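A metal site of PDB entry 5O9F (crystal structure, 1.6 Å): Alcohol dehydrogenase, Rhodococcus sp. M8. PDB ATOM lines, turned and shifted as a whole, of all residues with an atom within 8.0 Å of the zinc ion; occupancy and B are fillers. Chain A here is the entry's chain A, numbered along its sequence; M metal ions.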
ATOM      1  N   TRP A  90     -13.203 -28.423  -8.611  1.00  0.00           N
ATOM      2  CA  TRP A  90     -11.819 -28.074  -8.402  1.00  0.00           C
ATOM      3  C   TRP A  90     -11.287 -27.162  -9.503  1.00  0.00           C
ATOM      4  O   TRP A  90     -11.498 -27.420 -10.702  1.00  0.00           O
ATOM      5  CB  TRP A  90     -10.936 -29.318  -8.340  1.00  0.00           C
ATOM      6  CG  TRP A  90     -11.249 -30.230  -7.177  1.00  0.00           C
ATOM      7  CD1 TRP A  90     -12.080 -29.980  -6.125  1.00  0.00           C
ATOM      8  CD2 TRP A  90     -10.686 -31.519  -6.954  1.00  0.00           C
ATOM      9  NE1 TRP A  90     -12.090 -31.050  -5.266  1.00  0.00           N
ATOM     10  CE2 TRP A  90     -11.234 -32.009  -5.752  1.00  0.00           C
ATOM     11  CE3 TRP A  90      -9.782 -32.310  -7.664  1.00  0.00           C
ATOM     12  CZ2 TRP A  90     -10.939 -33.269  -5.253  1.00  0.00           C
ATOM     13  CZ3 TRP A  90      -9.466 -33.571  -7.159  1.00  0.00           C
ATOM     14  CH2 TRP A  90     -10.048 -34.034  -5.949  1.00  0.00           C
ATOM     15  N   GLY A  91     -10.633 -26.083  -9.082  1.00  0.00           N
ATOM     16  CA  GLY A  91      -9.943 -25.187  -9.998  1.00  0.00           C
ATOM     17  C   GLY A  91      -8.456 -25.163  -9.759  1.00  0.00           C
ATOM     18  O   GLY A  91      -7.920 -25.914  -8.924  1.00  0.00           O
ATOM     19  N   CYS A  92      -7.770 -24.274 -10.484  1.00  0.00           N
ATOM     20  CA  CYS A  92      -6.325 -24.190 -10.433  1.00  0.00           C
ATOM     21  C   CYS A  92      -5.794 -23.605  -9.116  1.00  0.00           C
ATOM     22  O   CYS A  92      -4.635 -23.817  -8.795  1.00  0.00           O
ATOM     23  CB  CYS A  92      -5.756 -23.411 -11.605  1.00  0.00           C
ATOM     24  SG  CYS A  92      -6.028 -21.595 -11.527  1.00  0.00           S
ATOM     25  N   GLY A  93      -6.620 -22.838  -8.435  1.00  0.00           N
ATOM     26  CA  GLY A  93      -6.245 -22.217  -7.156  1.00  0.00           C
ATOM     27  C   GLY A  93      -5.494 -20.898  -7.258  1.00  0.00           C
ATOM     28  O   GLY A  93      -5.268 -20.240  -6.232  1.00  0.00           O
ATOM     29  N   ALA A  94      -5.078 -20.512  -8.471  1.00  0.00           N
ATOM     30  CA  ALA A  94      -4.134 -19.411  -8.686  1.00  0.00           C
ATOM     31  C   ALA A  94      -4.638 -18.229  -9.510  1.00  0.00           C
ATOM     32  O   ALA A  94      -4.091 -17.129  -9.388  1.00  0.00           O
ATOM     33  CB  ALA A  94      -2.877 -19.955  -9.331  1.00  0.00           C
ATOM     34  N   CYS A  95      -5.627 -18.454 -10.380  1.00  0.00           N
ATOM     35  CA  CYS A  95      -6.126 -17.396 -11.245  1.00  0.00           C
ATOM     36  C   CYS A  95      -6.979 -16.415 -10.444  1.00  0.00           C
ATOM     37  O   CYS A  95      -7.275 -16.629  -9.254  1.00  0.00           O
ATOM     38  CB  CYS A  95      -6.984 -17.996 -12.375  1.00  0.00           C
ATOM     39  SG  CYS A  95      -8.533 -18.742 -11.872  1.00  0.00           S
ATOM     40  N   HIS A  96      -7.399 -15.350 -11.096  1.00  0.00           N
ATOM     41  CA  HIS A  96      -8.210 -14.314 -10.438  1.00  0.00           C
ATOM     42  C   HIS A  96      -9.524 -14.814  -9.841  1.00  0.00           C
ATOM     43  O   HIS A  96      -9.879 -14.473  -8.711  1.00  0.00           O
ATOM     44  CB  HIS A  96      -8.400 -13.141 -11.394  1.00  0.00           C
ATOM     45  CG  HIS A  96      -9.090 -11.959 -10.791  1.00  0.00           C
ATOM     46  ND1 HIS A  96     -10.450 -11.820 -10.809  1.00  0.00           N
ATOM     47  CD2 HIS A  96      -8.594 -10.819 -10.237  1.00  0.00           C
ATOM     48  CE1 HIS A  96     -10.780 -10.659 -10.250  1.00  0.00           C
ATOM     49  NE2 HIS A  96      -9.675 -10.037  -9.891  1.00  0.00           N
ATOM     50  N   ALA A  97     -10.245 -15.659 -10.577  1.00  0.00           N
ATOM     51  CA  ALA A  97     -11.429 -16.295 -10.035  1.00  0.00           C
ATOM     52  C   ALA A  97     -11.119 -17.192  -8.836  1.00  0.00           C
ATOM     53  O   ALA A  97     -11.765 -17.082  -7.773  1.00  0.00           O
ATOM     54  CB  ALA A  97     -12.112 -17.103 -11.126  1.00  0.00           C
ATOM     55  N   CYS A  98     -10.118 -18.048  -8.966  1.00  0.00           N
ATOM     56  CA  CYS A  98      -9.757 -18.950  -7.870  1.00  0.00           C
ATOM     57  C   CYS A  98      -9.275 -18.195  -6.637  1.00  0.00           C
ATOM     58  O   CYS A  98      -9.539 -18.631  -5.509  1.00  0.00           O
ATOM     59  CB  CYS A  98      -8.705 -19.978  -8.284  1.00  0.00           C
ATOM     60  SG  CYS A  98      -9.365 -21.282  -9.391  1.00  0.00           S
ATOM     61  N   ALA A  99      -8.597 -17.063  -6.854  1.00  0.00           N
ATOM     62  CA  ALA A  99      -8.107 -16.277  -5.716  1.00  0.00           C
ATOM     63  C   ALA A  99      -9.249 -15.770  -4.843  1.00  0.00           C
ATOM     64  O   ALA A  99      -9.052 -15.553  -3.632  1.00  0.00           O
ATOM     65  CB  ALA A  99      -7.227 -15.131  -6.184  1.00  0.00           C
ATOM     66  N   ARG A 102     -13.634 -18.663  -6.226  1.00  0.00           N
ATOM     67  CA  ARG A 102     -14.633 -18.932  -7.264  1.00  0.00           C
ATOM     68  C   ARG A 102     -14.097 -19.971  -8.243  1.00  0.00           C
ATOM     69  O   ARG A 102     -14.014 -19.762  -9.473  1.00  0.00           O
ATOM     70  CB  ARG A 102     -15.023 -17.629  -7.977  1.00  0.00           C
ATOM     71  CG  ARG A 102     -15.479 -16.547  -7.025  1.00  0.00           C
ATOM     72  CD  ARG A 102     -15.709 -15.218  -7.723  1.00  0.00           C
ATOM     73  NE  ARG A 102     -16.821 -15.263  -8.678  1.00  0.00           N
ATOM     74  CZ  ARG A 102     -18.111 -15.188  -8.357  1.00  0.00           C
ATOM     75  NH1 ARG A 102     -18.495 -15.127  -7.073  1.00  0.00           N
ATOM     76  NH2 ARG A 102     -19.039 -15.222  -9.303  1.00  0.00           N
ATOM     77  N   GLU A 103     -13.724 -21.127  -7.701  1.00  0.00           N
ATOM     78  CA  GLU A 103     -13.051 -22.151  -8.504  1.00  0.00           C
ATOM     79  C   GLU A 103     -14.014 -22.766  -9.524  1.00  0.00           C
ATOM     80  O   GLU A 103     -13.586 -23.342 -10.535  1.00  0.00           O
ATOM     81  CB  GLU A 103     -12.427 -23.222  -7.634  1.00  0.00           C
ATOM     82  CG  GLU A 103     -11.410 -22.651  -6.657  1.00  0.00           C
ATOM     83  CD  GLU A 103     -10.413 -23.666  -6.130  1.00  0.00           C
ATOM     84  OE1 GLU A 103     -10.387 -24.827  -6.575  1.00  0.00           O
ATOM     85  OE2 GLU A 103      -9.596 -23.252  -5.278  1.00  0.00           O
ATOM     86  N   ASN A 104     -15.294 -22.661  -9.234  1.00  0.00           N
ATOM     87  CA  ASN A 104     -16.352 -23.026 -10.180  1.00  0.00           C
ATOM     88  C   ASN A 104     -16.246 -22.293 -11.522  1.00  0.00           C
ATOM     89  O   ASN A 104     -16.684 -22.824 -12.550  1.00  0.00           O
ATOM     90  CB  ASN A 104     -17.747 -22.846  -9.562  1.00  0.00           C
ATOM     91  CG  ASN A 104     -18.011 -21.457  -9.028  1.00  0.00           C
ATOM     92  OD1 ASN A 104     -17.127 -20.808  -8.438  1.00  0.00           O
ATOM     93  ND2 ASN A 104     -19.264 -21.000  -9.177  1.00  0.00           N
ATOM     94  N   TYR A 105     -15.670 -21.087 -11.498  1.00  0.00           N
ATOM     95  CA  TYR A 105     -15.469 -20.287 -12.719  1.00  0.00           C
ATOM     96  C   TYR A 105     -14.012 -20.182 -13.136  1.00  0.00           C
ATOM     97  O   TYR A 105     -13.624 -19.280 -13.867  1.00  0.00           O
ATOM     98  CB  TYR A 105     -16.120 -18.893 -12.563  1.00  0.00           C
ATOM     99  CG  TYR A 105     -17.617 -18.944 -12.357  1.00  0.00           C
ATOM    100  CD1 TYR A 105     -18.442 -19.693 -13.216  1.00  0.00           C
ATOM    101  CD2 TYR A 105     -18.234 -18.213 -11.345  1.00  0.00           C
ATOM    102  CE1 TYR A 105     -19.807 -19.750 -13.029  1.00  0.00           C
ATOM    103  CE2 TYR A 105     -19.600 -18.263 -11.150  1.00  0.00           C
ATOM    104  CZ  TYR A 105     -20.404 -19.050 -12.007  1.00  0.00           C
ATOM    105  OH  TYR A 105     -21.766 -19.112 -11.842  1.00  0.00           O
ATOM    106  N   CYS A 106     -13.168 -21.129 -12.685  1.00  0.00           N
ATOM    107  CA  CYS A 106     -11.785 -21.188 -13.151  1.00  0.00           C
ATOM    108  C   CYS A 106     -11.758 -21.527 -14.667  1.00  0.00           C
ATOM    109  O   CYS A 106     -12.427 -22.449 -15.101  1.00  0.00           O
ATOM    110  CB  CYS A 106     -11.067 -22.292 -12.403  1.00  0.00           C
ATOM    111  SG  CYS A 106      -9.337 -22.482 -12.838  1.00  0.00           S
ATOM    112  N   THR A 107     -10.979 -20.806 -15.452  1.00  0.00           N
ATOM    113  CA  THR A 107     -10.822 -21.179 -16.878  1.00  0.00           C
ATOM    114  C   THR A 107      -9.512 -21.895 -17.172  1.00  0.00           C
ATOM    115  O   THR A 107      -9.276 -22.319 -18.333  1.00  0.00           O
ATOM    116  CB  THR A 107     -10.868 -19.922 -17.749  1.00  0.00           C
ATOM    117  OG1 THR A 107      -9.764 -19.092 -17.426  1.00  0.00           O
ATOM    118  CG2 THR A 107     -12.157 -19.156 -17.489  1.00  0.00           C
ATOM    119  N   ARG A 108      -8.674 -22.067 -16.141  1.00  0.00           N
ATOM    120  CA  ARG A 108      -7.374 -22.698 -16.304  1.00  0.00           C
ATOM    121  C   ARG A 108      -7.376 -24.195 -15.990  1.00  0.00           C
ATOM    122  O   ARG A 108      -6.415 -24.874 -16.348  1.00  0.00           O
ATOM    123  CB  ARG A 108      -6.344 -22.005 -15.430  1.00  0.00           C
ATOM    124  CG  ARG A 108      -6.212 -20.504 -15.652  1.00  0.00           C
ATOM    125  CD  ARG A 108      -4.942 -20.110 -16.372  1.00  0.00           C
ATOM    126  NE  ARG A 108      -3.717 -20.596 -15.705  1.00  0.00           N
ATOM    127  CZ  ARG A 108      -2.836 -21.497 -16.189  1.00  0.00           C
ATOM    128  NH1 ARG A 108      -1.784 -21.820 -15.448  1.00  0.00           N
ATOM    129  NH2 ARG A 108      -2.998 -22.049 -17.392  1.00  0.00           N
ATOM    130  N   ALA A 109      -8.418 -24.705 -15.335  1.00  0.00           N
ATOM    131  CA  ALA A 109      -8.401 -26.067 -14.813  1.00  0.00           C
ATOM    132  C   ALA A 109      -8.215 -27.122 -15.902  1.00  0.00           C
ATOM    133  O   ALA A 109      -7.363 -28.003 -15.769  1.00  0.00           O
ATOM    134  CB  ALA A 109      -9.678 -26.340 -14.016  1.00  0.00           C
ATOM    135  N   LEU A 112      -4.727 -27.453 -17.330  1.00  0.00           N
ATOM    136  CA  LEU A 112      -3.836 -28.036 -16.339  1.00  0.00           C
ATOM    137  C   LEU A 112      -4.169 -29.505 -15.996  1.00  0.00           C
ATOM    138  O   LEU A 112      -3.490 -30.103 -15.156  1.00  0.00           O
ATOM    139  CB  LEU A 112      -3.817 -27.171 -15.069  1.00  0.00           C
ATOM    140  CG  LEU A 112      -3.242 -25.763 -15.274  1.00  0.00           C
ATOM    141  CD1 LEU A 112      -3.534 -24.874 -14.073  1.00  0.00           C
ATOM    142  CD2 LEU A 112      -1.750 -25.826 -15.521  1.00  0.00           C
ATOM    143  N   ILE A 114      -6.893 -30.610 -14.462  1.00  0.00           N
ATOM    144  CA  ILE A 114      -7.600 -30.669 -13.193  1.00  0.00           C
ATOM    145  C   ILE A 114      -9.048 -30.994 -13.478  1.00  0.00           C
ATOM    146  O   ILE A 114      -9.740 -30.239 -14.146  1.00  0.00           O
ATOM    147  CB  ILE A 114      -7.486 -29.342 -12.405  1.00  0.00           C
ATOM    148  CG1 ILE A 114      -6.025 -29.068 -12.043  1.00  0.00           C
ATOM    149  CG2 ILE A 114      -8.375 -29.382 -11.148  1.00  0.00           C
ATOM    150  CD1 ILE A 114      -5.764 -27.661 -11.536  1.00  0.00           C
ATOM    151  N   ARG A 135      -7.470 -27.191   0.644  1.00  0.00           N
ATOM    152  CA  ARG A 135      -8.427 -26.129   0.368  1.00  0.00           C
ATOM    153  C   ARG A 135      -9.749 -26.646  -0.187  1.00  0.00           C
ATOM    154  O   ARG A 135     -10.710 -25.891  -0.269  1.00  0.00           O
ATOM    155  CB  ARG A 135      -7.837 -25.047  -0.556  1.00  0.00           C
ATOM    156  CG  ARG A 135      -7.866 -25.371  -2.044  1.00  0.00           C
ATOM    157  CD  ARG A 135      -7.202 -24.260  -2.857  1.00  0.00           C
ATOM    158  NE  ARG A 135      -7.381 -24.540  -4.283  1.00  0.00           N
ATOM    159  CZ  ARG A 135      -6.621 -25.362  -5.013  1.00  0.00           C
ATOM    160  NH1 ARG A 135      -5.578 -25.978  -4.496  1.00  0.00           N
ATOM    161  NH2 ARG A 135      -6.929 -25.538  -6.301  1.00  0.00           N
HETATM  162 ZN    ZN M   1      -8.269 -20.992 -11.444  1.00  0.00          ZN
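N of Arg 108 sits close to SG of Cys 106 (3.4 Å). The backbone NH of Ala 109 sits close to the side-chain sulfur of Cys 106, at 3.5 Å. The side-chain sulfur (SG) of Cys 95 sits close to the backbone NH (N) of Ala 97. The backbone NH (N) of Ala 94 sits close to the side-chain sulfur (SG) of Cys 92. The backbone NH of Gly 93 sits close to the side-chain sulfur of Cys 98 (3.3 Å).
Merely in contact with the zinc ion: Gly 93 (3.9 Å).
The zinc ion is bound by the side-chain sulfur of Cys 106 (2.3 Å), the side-chain sulfur of Cys 95 (2.3 Å), the side-chain sulfur of Cys 92 (2.3 Å) and the side-chain sulfur of Cys 98 (2.3 Å). The zinc ion has four donor atoms within binding distance.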
